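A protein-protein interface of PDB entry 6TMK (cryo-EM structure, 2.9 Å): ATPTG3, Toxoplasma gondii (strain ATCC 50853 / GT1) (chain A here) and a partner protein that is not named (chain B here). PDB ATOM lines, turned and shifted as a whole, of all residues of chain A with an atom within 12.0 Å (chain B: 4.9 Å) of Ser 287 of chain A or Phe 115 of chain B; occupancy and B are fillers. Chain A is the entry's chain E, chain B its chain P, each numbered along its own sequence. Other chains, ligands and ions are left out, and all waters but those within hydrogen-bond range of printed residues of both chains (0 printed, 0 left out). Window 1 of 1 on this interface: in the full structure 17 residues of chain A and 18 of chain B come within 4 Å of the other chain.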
ATOM      1  N   ALA A 276      23.290 -11.727  -9.893  1.00  0.00           N
ATOM      2  CA  ALA A 276      22.041 -11.209  -9.367  1.00  0.00           C
ATOM      3  C   ALA A 276      21.538 -12.036  -8.196  1.00  0.00           C
ATOM      4  O   ALA A 276      20.810 -11.512  -7.349  1.00  0.00           O
ATOM      5  CB  ALA A 276      20.994 -11.168 -10.475  1.00  0.00           C
ATOM      6  N   ALA A 277      21.929 -13.307  -8.118  1.00  0.00           N
ATOM      7  CA  ALA A 277      21.511 -14.147  -7.005  1.00  0.00           C
ATOM      8  C   ALA A 277      22.183 -13.703  -5.715  1.00  0.00           C
ATOM      9  O   ALA A 277      21.531 -13.561  -4.673  1.00  0.00           O
ATOM     10  CB  ALA A 277      21.834 -15.604  -7.307  1.00  0.00           C
ATOM     11  N   ALA A 278      23.498 -13.491  -5.764  1.00  0.00           N
ATOM     12  CA  ALA A 278      24.220 -13.000  -4.600  1.00  0.00           C
ATOM     13  C   ALA A 278      23.732 -11.618  -4.194  1.00  0.00           C
ATOM     14  O   ALA A 278      23.596 -11.324  -3.002  1.00  0.00           O
ATOM     15  CB  ALA A 278      25.712 -12.975  -4.895  1.00  0.00           C
ATOM     16  N   THR A 279      23.468 -10.751  -5.172  1.00  0.00           N
ATOM     17  CA  THR A 279      22.980  -9.415  -4.862  1.00  0.00           C
ATOM     18  C   THR A 279      21.605  -9.476  -4.212  1.00  0.00           C
ATOM     19  O   THR A 279      21.322  -8.734  -3.264  1.00  0.00           O
ATOM     20  CB  THR A 279      22.941  -8.570  -6.135  1.00  0.00           C
ATOM     21  OG1 THR A 279      24.196  -8.663  -6.813  1.00  0.00           O
ATOM     22  CG2 THR A 279      22.653  -7.119  -5.816  1.00  0.00           C
ATOM     23  N   ALA A 280      20.739 -10.361  -4.703  1.00  0.00           N
ATOM     24  CA  ALA A 280      19.425 -10.527  -4.101  1.00  0.00           C
ATOM     25  C   ALA A 280      19.530 -11.064  -2.681  1.00  0.00           C
ATOM     26  O   ALA A 280      18.812 -10.611  -1.782  1.00  0.00           O
ATOM     27  CB  ALA A 280      18.589 -11.463  -4.963  1.00  0.00           C
ATOM     28  N   PHE A 281      20.410 -12.040  -2.462  1.00  0.00           N
ATOM     29  CA  PHE A 281      20.639 -12.554  -1.118  1.00  0.00           C
ATOM     30  C   PHE A 281      21.115 -11.449  -0.186  1.00  0.00           C
ATOM     31  O   PHE A 281      20.665 -11.347   0.963  1.00  0.00           O
ATOM     32  CB  PHE A 281      21.646 -13.695  -1.186  1.00  0.00           C
ATOM     33  CG  PHE A 281      21.935 -14.333   0.132  1.00  0.00           C
ATOM     34  CD1 PHE A 281      20.980 -15.093   0.768  1.00  0.00           C
ATOM     35  CD2 PHE A 281      23.172 -14.199   0.721  1.00  0.00           C
ATOM     36  CE1 PHE A 281      21.244 -15.681   1.970  1.00  0.00           C
ATOM     37  CE2 PHE A 281      23.439 -14.789   1.924  1.00  0.00           C
ATOM     38  CZ  PHE A 281      22.477 -15.535   2.548  1.00  0.00           C
ATOM     39  N   ARG A 282      22.038 -10.620  -0.668  1.00  0.00           N
ATOM     40  CA  ARG A 282      22.531  -9.500   0.119  1.00  0.00           C
ATOM     41  C   ARG A 282      21.407  -8.533   0.460  1.00  0.00           C
ATOM     42  O   ARG A 282      21.325  -8.035   1.587  1.00  0.00           O
ATOM     43  CB  ARG A 282      23.639  -8.796  -0.654  1.00  0.00           C
ATOM     44  CG  ARG A 282      24.494  -7.878   0.160  1.00  0.00           C
ATOM     45  CD  ARG A 282      25.618  -7.343  -0.682  1.00  0.00           C
ATOM     46  NE  ARG A 282      26.638  -8.359  -0.908  1.00  0.00           N
ATOM     47  CZ  ARG A 282      27.916  -8.093  -1.151  1.00  0.00           C
ATOM     48  NH1 ARG A 282      28.340  -6.842  -1.208  1.00  0.00           N
ATOM     49  NH2 ARG A 282      28.771  -9.084  -1.339  1.00  0.00           N
ATOM     50  N   ALA A 283      20.519  -8.272  -0.498  1.00  0.00           N
ATOM     51  CA  ALA A 283      19.387  -7.389  -0.245  1.00  0.00           C
ATOM     52  C   ALA A 283      18.432  -7.982   0.784  1.00  0.00           C
ATOM     53  O   ALA A 283      17.865  -7.256   1.608  1.00  0.00           O
ATOM     54  CB  ALA A 283      18.655  -7.115  -1.549  1.00  0.00           C
ATOM     55  N   VAL A 284      18.235  -9.297   0.747  1.00  0.00           N
ATOM     56  CA  VAL A 284      17.347  -9.942   1.707  1.00  0.00           C
ATOM     57  C   VAL A 284      17.927  -9.848   3.111  1.00  0.00           C
ATOM     58  O   VAL A 284      17.219  -9.542   4.082  1.00  0.00           O
ATOM     59  CB  VAL A 284      17.102 -11.403   1.297  1.00  0.00           C
ATOM     60  CG1 VAL A 284      16.396 -12.148   2.398  1.00  0.00           C
ATOM     61  CG2 VAL A 284      16.307 -11.458   0.031  1.00  0.00           C
ATOM     62  N   LEU A 285      19.222 -10.136   3.244  1.00  0.00           N
ATOM     63  CA  LEU A 285      19.885  -9.962   4.529  1.00  0.00           C
ATOM     64  C   LEU A 285      19.769  -8.524   5.003  1.00  0.00           C
ATOM     65  O   LEU A 285      19.553  -8.263   6.192  1.00  0.00           O
ATOM     66  CB  LEU A 285      21.351 -10.359   4.422  1.00  0.00           C
ATOM     67  CG  LEU A 285      21.686 -11.797   4.051  1.00  0.00           C
ATOM     68  CD1 LEU A 285      23.150 -12.015   4.285  1.00  0.00           C
ATOM     69  CD2 LEU A 285      20.878 -12.798   4.828  1.00  0.00           C
ATOM     70  N   GLU A 286      19.920  -7.581   4.079  1.00  0.00           N
ATOM     71  CA  GLU A 286      19.786  -6.169   4.397  1.00  0.00           C
ATOM     72  C   GLU A 286      18.411  -5.865   4.975  1.00  0.00           C
ATOM     73  O   GLU A 286      18.288  -5.172   5.992  1.00  0.00           O
ATOM     74  CB  GLU A 286      20.041  -5.363   3.130  1.00  0.00           C
ATOM     75  CG  GLU A 286      20.242  -3.909   3.337  1.00  0.00           C
ATOM     76  CD  GLU A 286      20.693  -3.206   2.075  1.00  0.00           C
ATOM     77  OE1 GLU A 286      21.617  -3.721   1.410  1.00  0.00           O
ATOM     78  OE2 GLU A 286      20.125  -2.144   1.745  1.00  0.00           O
ATOM     79  N   SER A 287      17.365  -6.395   4.347  1.00  0.00           N
ATOM     80  CA  SER A 287      16.006  -6.139   4.808  1.00  0.00           C
ATOM     81  C   SER A 287      15.770  -6.732   6.191  1.00  0.00           C
ATOM     82  O   SER A 287      15.180  -6.083   7.066  1.00  0.00           O
ATOM     83  CB  SER A 287      15.011  -6.709   3.804  1.00  0.00           C
ATOM     84  OG  SER A 287      13.723  -6.815   4.372  1.00  0.00           O
ATOM     85  N   ALA A 288      16.209  -7.970   6.405  1.00  0.00           N
ATOM     86  CA  ALA A 288      16.017  -8.597   7.709  1.00  0.00           C
ATOM     87  C   ALA A 288      16.769  -7.845   8.804  1.00  0.00           C
ATOM     88  O   ALA A 288      16.235  -7.613   9.902  1.00  0.00           O
ATOM     89  CB  ALA A 288      16.466 -10.050   7.645  1.00  0.00           C
ATOM     90  N   TRP A 289      18.011  -7.451   8.520  1.00  0.00           N
ATOM     91  CA  TRP A 289      18.778  -6.651   9.463  1.00  0.00           C
ATOM     92  C   TRP A 289      18.073  -5.338   9.768  1.00  0.00           C
ATOM     93  O   TRP A 289      18.067  -4.880  10.917  1.00  0.00           O
ATOM     94  CB  TRP A 289      20.170  -6.403   8.891  1.00  0.00           C
ATOM     95  CG  TRP A 289      21.145  -5.868   9.864  1.00  0.00           C
ATOM     96  CD1 TRP A 289      21.743  -6.546  10.876  1.00  0.00           C
ATOM     97  CD2 TRP A 289      21.656  -4.537   9.916  1.00  0.00           C
ATOM     98  NE1 TRP A 289      22.593  -5.721  11.562  1.00  0.00           N
ATOM     99  CE2 TRP A 289      22.558  -4.478  10.989  1.00  0.00           C
ATOM    100  CE3 TRP A 289      21.438  -3.387   9.158  1.00  0.00           C
ATOM    101  CZ2 TRP A 289      23.237  -3.318  11.325  1.00  0.00           C
ATOM    102  CZ3 TRP A 289      22.112  -2.238   9.495  1.00  0.00           C
ATOM    103  CH2 TRP A 289      23.001  -2.211  10.567  1.00  0.00           C
ATOM    104  N   LYS A 290      17.480  -4.713   8.753  1.00  0.00           N
ATOM    105  CA  LYS A 290      16.773  -3.459   8.970  1.00  0.00           C
ATOM    106  C   LYS A 290      15.564  -3.664   9.868  1.00  0.00           C
ATOM    107  O   LYS A 290      15.268  -2.825  10.723  1.00  0.00           O
ATOM    108  CB  LYS A 290      16.358  -2.852   7.636  1.00  0.00           C
ATOM    109  CG  LYS A 290      17.406  -1.958   7.038  1.00  0.00           C
ATOM    110  CD  LYS A 290      16.877  -1.180   5.865  1.00  0.00           C
ATOM    111  CE  LYS A 290      16.832  -2.014   4.623  1.00  0.00           C
ATOM    112  NZ  LYS A 290      16.813  -1.160   3.420  1.00  0.00           N
ATOM    113  N   CYS A 291      14.860  -4.779   9.695  1.00  0.00           N
ATOM    114  CA  CYS A 291      13.744  -5.093  10.584  1.00  0.00           C
ATOM    115  C   CYS A 291      14.214  -5.195  12.030  1.00  0.00           C
ATOM    116  O   CYS A 291      13.631  -4.586  12.942  1.00  0.00           O
ATOM    117  CB  CYS A 291      13.086  -6.399  10.146  1.00  0.00           C
ATOM    118  SG  CYS A 291      12.007  -6.274   8.706  1.00  0.00           S
ATOM    119  N   ASP A 292      15.282  -5.960  12.256  1.00  0.00           N
ATOM    120  CA  ASP A 292      15.789  -6.135  13.615  1.00  0.00           C
ATOM    121  C   ASP A 292      16.220  -4.801  14.221  1.00  0.00           C
ATOM    122  O   ASP A 292      15.907  -4.497  15.381  1.00  0.00           O
ATOM    123  CB  ASP A 292      16.948  -7.124  13.613  1.00  0.00           C
ATOM    124  CG  ASP A 292      16.524  -8.520  13.212  1.00  0.00           C
ATOM    125  OD1 ASP A 292      15.360  -8.886  13.472  1.00  0.00           O
ATOM    126  OD2 ASP A 292      17.357  -9.255  12.641  1.00  0.00           O
ATOM    127  N   ILE A 293      16.946  -3.991  13.450  1.00  0.00           N
ATOM    128  CA  ILE A 293      17.437  -2.725  13.979  1.00  0.00           C
ATOM    129  C   ILE A 293      16.299  -1.743  14.205  1.00  0.00           C
ATOM    130  O   ILE A 293      16.369  -0.909  15.113  1.00  0.00           O
ATOM    131  CB  ILE A 293      18.492  -2.139  13.029  1.00  0.00           C
ATOM    132  CG1 ILE A 293      19.704  -3.061  12.950  1.00  0.00           C
ATOM    133  CG2 ILE A 293      18.905  -0.764  13.486  1.00  0.00           C
ATOM    134  CD1 ILE A 293      20.420  -3.259  14.250  1.00  0.00           C
ATOM    135  N   ASP A 294      15.230  -1.826  13.415  1.00  0.00           N
ATOM    136  CA  ASP A 294      14.066  -0.992  13.674  1.00  0.00           C
ATOM    137  C   ASP A 294      13.416  -1.370  14.996  1.00  0.00           C
ATOM    138  O   ASP A 294      13.018  -0.495  15.774  1.00  0.00           O
ATOM    139  CB  ASP A 294      13.070  -1.114  12.526  1.00  0.00           C
ATOM    140  CG  ASP A 294      11.964  -0.085  12.604  1.00  0.00           C
ATOM    141  OD1 ASP A 294      11.974   0.730  13.551  1.00  0.00           O
ATOM    142  OD2 ASP A 294      11.084  -0.087  11.718  1.00  0.00           O
ATOM    143  N   GLU A 295      13.307  -2.671  15.268  1.00  0.00           N
ATOM    144  CA  GLU A 295      12.792  -3.105  16.565  1.00  0.00           C
ATOM    145  C   GLU A 295      13.652  -2.575  17.707  1.00  0.00           C
ATOM    146  O   GLU A 295      13.136  -2.082  18.721  1.00  0.00           O
ATOM    147  CB  GLU A 295      12.723  -4.627  16.616  1.00  0.00           C
ATOM    148  CG  GLU A 295      11.464  -5.205  16.010  1.00  0.00           C
ATOM    149  CD  GLU A 295      11.380  -6.708  16.171  1.00  0.00           C
ATOM    150  OE1 GLU A 295      12.392  -7.321  16.573  1.00  0.00           O
ATOM    151  OE2 GLU A 295      10.302  -7.277  15.898  1.00  0.00           O
ATOM    152  N   GLN A 296      14.974  -2.693  17.569  1.00  0.00           N
ATOM    153  CA  GLN A 296      15.863  -2.211  18.622  1.00  0.00           C
ATOM    154  C   GLN A 296      15.731  -0.707  18.822  1.00  0.00           C
ATOM    155  O   GLN A 296      15.707  -0.225  19.960  1.00  0.00           O
ATOM    156  CB  GLN A 296      17.309  -2.574  18.294  1.00  0.00           C
ATOM    157  CG  GLN A 296      17.618  -4.047  18.438  1.00  0.00           C
ATOM    158  CD  GLN A 296      19.051  -4.374  18.083  1.00  0.00           C
ATOM    159  OE1 GLN A 296      19.977  -3.669  18.483  1.00  0.00           O
ATOM    160  NE2 GLN A 296      19.241  -5.447  17.326  1.00  0.00           N
ATOM    161  N   LYS A 298      13.071   1.065  18.241  1.00  0.00           N
ATOM    162  CA  LYS A 298      11.780   1.311  18.873  1.00  0.00           C
ATOM    163  C   LYS A 298      11.863   1.092  20.374  1.00  0.00           C
ATOM    164  O   LYS A 298      11.435   1.942  21.165  1.00  0.00           O
ATOM    165  CB  LYS A 298      10.707   0.409  18.267  1.00  0.00           C
ATOM    166  CG  LYS A 298      10.132   0.923  16.968  1.00  0.00           C
ATOM    167  CD  LYS A 298       8.829   0.223  16.629  1.00  0.00           C
ATOM    168  CE  LYS A 298       9.062  -1.188  16.125  1.00  0.00           C
ATOM    169  NZ  LYS A 298       9.681  -1.204  14.773  1.00  0.00           N
ATOM    170  N   ARG B  75       9.114  -8.867  -7.262  1.00  0.00           N
ATOM    171  CA  ARG B  75      10.266  -8.792  -6.371  1.00  0.00           C
ATOM    172  C   ARG B  75      10.439 -10.085  -5.589  1.00  0.00           C
ATOM    173  O   ARG B  75      11.541 -10.649  -5.520  1.00  0.00           O
ATOM    174  CB  ARG B  75      10.104  -7.622  -5.407  1.00  0.00           C
ATOM    175  CG  ARG B  75      10.236  -6.261  -6.028  1.00  0.00           C
ATOM    176  CD  ARG B  75      10.728  -5.257  -5.014  1.00  0.00           C
ATOM    177  NE  ARG B  75       9.818  -5.111  -3.884  1.00  0.00           N
ATOM    178  CZ  ARG B  75       8.749  -4.322  -3.884  1.00  0.00           C
ATOM    179  NH1 ARG B  75       8.444  -3.614  -4.957  1.00  0.00           N
ATOM    180  NH2 ARG B  75       7.978  -4.249  -2.814  1.00  0.00           N
ATOM    181  N   ALA B  79      13.511 -12.876  -5.751  1.00  0.00           N
ATOM    182  CA  ALA B  79      14.318 -13.287  -4.608  1.00  0.00           C
ATOM    183  C   ALA B  79      14.216 -14.789  -4.370  1.00  0.00           C
ATOM    184  O   ALA B  79      15.216 -15.449  -4.049  1.00  0.00           O
ATOM    185  CB  ALA B  79      13.888 -12.515  -3.369  1.00  0.00           C
ATOM    186  N   LEU B 106       9.673 -14.088   2.846  1.00  0.00           N
ATOM    187  CA  LEU B 106      10.233 -13.015   2.036  1.00  0.00           C
ATOM    188  C   LEU B 106       9.218 -11.905   1.806  1.00  0.00           C
ATOM    189  O   LEU B 106       9.576 -10.724   1.774  1.00  0.00           O
ATOM    190  CB  LEU B 106      10.721 -13.572   0.706  1.00  0.00           C
ATOM    191  CG  LEU B 106      11.790 -14.654   0.794  1.00  0.00           C
ATOM    192  CD1 LEU B 106      11.985 -15.271  -0.563  1.00  0.00           C
ATOM    193  CD2 LEU B 106      13.089 -14.109   1.324  1.00  0.00           C
ATOM    194  N   TYR B 109       9.174  -9.757   4.952  1.00  0.00           N
ATOM    195  CA  TYR B 109      10.344  -8.888   4.984  1.00  0.00           C
ATOM    196  C   TYR B 109      10.219  -7.756   3.974  1.00  0.00           C
ATOM    197  O   TYR B 109      10.623  -6.624   4.252  1.00  0.00           O
ATOM    198  CB  TYR B 109      11.617  -9.683   4.712  1.00  0.00           C
ATOM    199  CG  TYR B 109      11.958 -10.722   5.748  1.00  0.00           C
ATOM    200  CD1 TYR B 109      11.239 -10.826   6.923  1.00  0.00           C
ATOM    201  CD2 TYR B 109      13.015 -11.592   5.553  1.00  0.00           C
ATOM    202  CE1 TYR B 109      11.551 -11.774   7.863  1.00  0.00           C
ATOM    203  CE2 TYR B 109      13.336 -12.538   6.490  1.00  0.00           C
ATOM    204  CZ  TYR B 109      12.603 -12.625   7.643  1.00  0.00           C
ATOM    205  OH  TYR B 109      12.927 -13.573   8.579  1.00  0.00           O
ATOM    206  N   ASP B 110       9.668  -8.041   2.795  1.00  0.00           N
ATOM    207  CA  ASP B 110       9.580  -7.020   1.759  1.00  0.00           C
ATOM    208  C   ASP B 110       8.543  -5.962   2.104  1.00  0.00           C
ATOM    209  O   ASP B 110       8.768  -4.770   1.871  1.00  0.00           O
ATOM    210  CB  ASP B 110       9.251  -7.671   0.419  1.00  0.00           C
ATOM    211  CG  ASP B 110       9.234  -6.683  -0.723  1.00  0.00           C
ATOM    212  OD1 ASP B 110      10.317  -6.205  -1.117  1.00  0.00           O
ATOM    213  OD2 ASP B 110       8.135  -6.383  -1.233  1.00  0.00           O
ATOM    214  N   HIS B 113      10.258  -3.847   4.916  1.00  0.00           N
ATOM    215  CA  HIS B 113      11.325  -3.066   4.297  1.00  0.00           C
ATOM    216  C   HIS B 113      11.535  -3.602   2.889  1.00  0.00           C
ATOM    217  O   HIS B 113      12.070  -4.719   2.733  1.00  0.00           O
ATOM    218  CB  HIS B 113      12.612  -3.171   5.105  1.00  0.00           C
ATOM    219  CG  HIS B 113      12.658  -2.265   6.291  1.00  0.00           C
ATOM    220  ND1 HIS B 113      12.300  -2.680   7.555  1.00  0.00           N
ATOM    221  CD2 HIS B 113      13.017  -0.966   6.409  1.00  0.00           C
ATOM    222  CE1 HIS B 113      12.436  -1.675   8.401  1.00  0.00           C
ATOM    223  NE2 HIS B 113      12.870  -0.623   7.730  1.00  0.00           N
ATOM    224  N   PRO B 114      11.153  -2.866   1.847  1.00  0.00           N
ATOM    225  CA  PRO B 114      11.217  -3.429   0.495  1.00  0.00           C
ATOM    226  C   PRO B 114      12.636  -3.767   0.072  1.00  0.00           C
ATOM    227  O   PRO B 114      13.619  -3.237   0.595  1.00  0.00           O
ATOM    228  CB  PRO B 114      10.625  -2.318  -0.378  1.00  0.00           C
ATOM    229  CG  PRO B 114       9.791  -1.526   0.538  1.00  0.00           C
ATOM    230  CD  PRO B 114      10.510  -1.544   1.844  1.00  0.00           C
ATOM    231  N   PHE B 115      12.729  -4.671  -0.897  1.00  0.00           N
ATOM    232  CA  PHE B 115      14.016  -5.099  -1.417  1.00  0.00           C
ATOM    233  C   PHE B 115      14.534  -4.133  -2.469  1.00  0.00           C
ATOM    234  O   PHE B 115      13.769  -3.503  -3.205  1.00  0.00           O
ATOM    235  CB  PHE B 115      13.934  -6.491  -2.034  1.00  0.00           C
ATOM    236  CG  PHE B 115      13.548  -7.571  -1.076  1.00  0.00           C
ATOM    237  CD1 PHE B 115      13.873  -7.486   0.260  1.00  0.00           C
ATOM    238  CD2 PHE B 115      12.879  -8.687  -1.522  1.00  0.00           C
ATOM    239  CE1 PHE B 115      13.522  -8.486   1.129  1.00  0.00           C
ATOM    240  CE2 PHE B 115      12.529  -9.686  -0.658  1.00  0.00           C
ATOM    241  CZ  PHE B 115      12.852  -9.586   0.669  1.00  0.00           C
ATOM    242  N   VAL B 116      15.854  -4.035  -2.537  1.00  0.00           N
ATOM    243  CA  VAL B 116      16.549  -3.231  -3.529  1.00  0.00           C
ATOM    244  C   VAL B 116      17.515  -4.178  -4.224  1.00  0.00           C
ATOM    245  O   VAL B 116      18.624  -4.423  -3.734  1.00  0.00           O
ATOM    246  CB  VAL B 116      17.280  -2.042  -2.907  1.00  0.00           C
ATOM    247  CG1 VAL B 116      18.073  -1.311  -3.966  1.00  0.00           C
ATOM    248  CG2 VAL B 116      16.295  -1.120  -2.229  1.00  0.00           C
ATOM    249  N   LEU B 117      17.101  -4.714  -5.366  1.00  0.00           N
ATOM    250  CA  LEU B 117      17.799  -5.823  -5.991  1.00  0.00           C
ATOM    251  C   LEU B 117      18.816  -5.380  -7.028  1.00  0.00           C
ATOM    252  O   LEU B 117      19.657  -6.189  -7.433  1.00  0.00           O
ATOM    253  CB  LEU B 117      16.787  -6.761  -6.643  1.00  0.00           C
ATOM    254  CG  LEU B 117      15.747  -7.340  -5.689  1.00  0.00           C
ATOM    255  CD1 LEU B 117      14.486  -7.686  -6.431  1.00  0.00           C
ATOM    256  CD2 LEU B 117      16.284  -8.547  -4.971  1.00  0.00           C
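The side-chain hydroxyl of Ser 287 of chain A sits at hydrogen-bond distance from the backbone carbonyl oxygen of Tyr 109 of chain B.
The backbone carbonyl oxygen of His 113 of chain B lies within hydrogen-bond range of the side-chain hydroxyl of Ser 287 of chain A (3.1 Å).
The side-chain sulfur (SG) of Cys 291 of chain A lies within hydrogen-bond range of a ring nitrogen (ND1) of His 113 of chain B (3.8 Å).
OE2 of Glu 286 of chain A is in salt-bridge range of NZ of Lys 290 of chain A, 3.8 Å away.
SG of Cys 291 of chain A sits at hydrogen-bond distance from O of Ser 287 of chain A (3.6 Å).
OD1 of Asp 294 of chain A lies within salt-bridge range of NZ of Lys 298 of chain A.
The side-chain carboxylate (OD1) of Asp 110 of chain B sits at hydrogen-bond distance from the backbone NH (N) of Phe 115 of chain B (2.9 Å).
Among the printed residues, pairs that only touch across the chains: Ala 283 of chain A with Val 116 of chain B, Thr 279 of chain A with Leu 117 of chain B, Ser 287 of chain A with Phe 115 of chain B, Ala 280 of chain A with Leu 117 of chain B, Lys 290 of chain A with His 113 of chain B, Asp 294 of chain A with His 113 of chain B, Val 284 of chain A with Phe 115 of chain B and Val 284 of chain A with Leu 106 of chain B.
Ser 287 of chain A touches just these residues of chain B: Tyr 109 (3.1 Å), His 113 (3.1 Å) and Phe 115 (3.5 Å).
Of the printed residues of chain A, Phe 115 of chain B touches Val 284 and Ser 287.
No residue of chain A comes within 4 Å of Arg 75 of chain B.
No residue of chain A comes within 4 Å of Ala 79 of chain B.
Tyr 109 of chain B touches just one residue of chain A: Ser 287 (3.1 Å).
No residue of chain A comes within 4 Å of Asp 110 of chain B.
His 113 of chain B touches just these residues of chain A: Ser 287, Lys 290, Cys 291 and Asp 294.
Val 116 of chain B touches just one residue of chain A: Ala 283.
Of the printed residues of chain A, Leu 117 of chain B touches Thr 279 and Ala 280.
Of the printed residues of chain B, Val 284 of chain A touches Leu 106 and Phe 115.
Of the printed residues of chain B, Ala 280 of chain A touches Leu 117.
Asp 292 of chain A touches none of the printed residues of chain B.
Of the 22 printed residues of chain A, 8 touch a printed residue of chain B.
Hydrophobic or aromatic side chains of chain A within 4 Å of the printed part of chain B: Ala 280, Ala 283 and Val 284.
Hydrophobic or aromatic side chains of chain B within 4 Å of the printed part of chain A: Leu 106, Tyr 109, His 113, Phe 115 and Leu 117.
Among the printed residues, no Asp or Glu carboxylate lies within 4 Å of a Lys or Arg side-chain nitrogen of the other chain.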
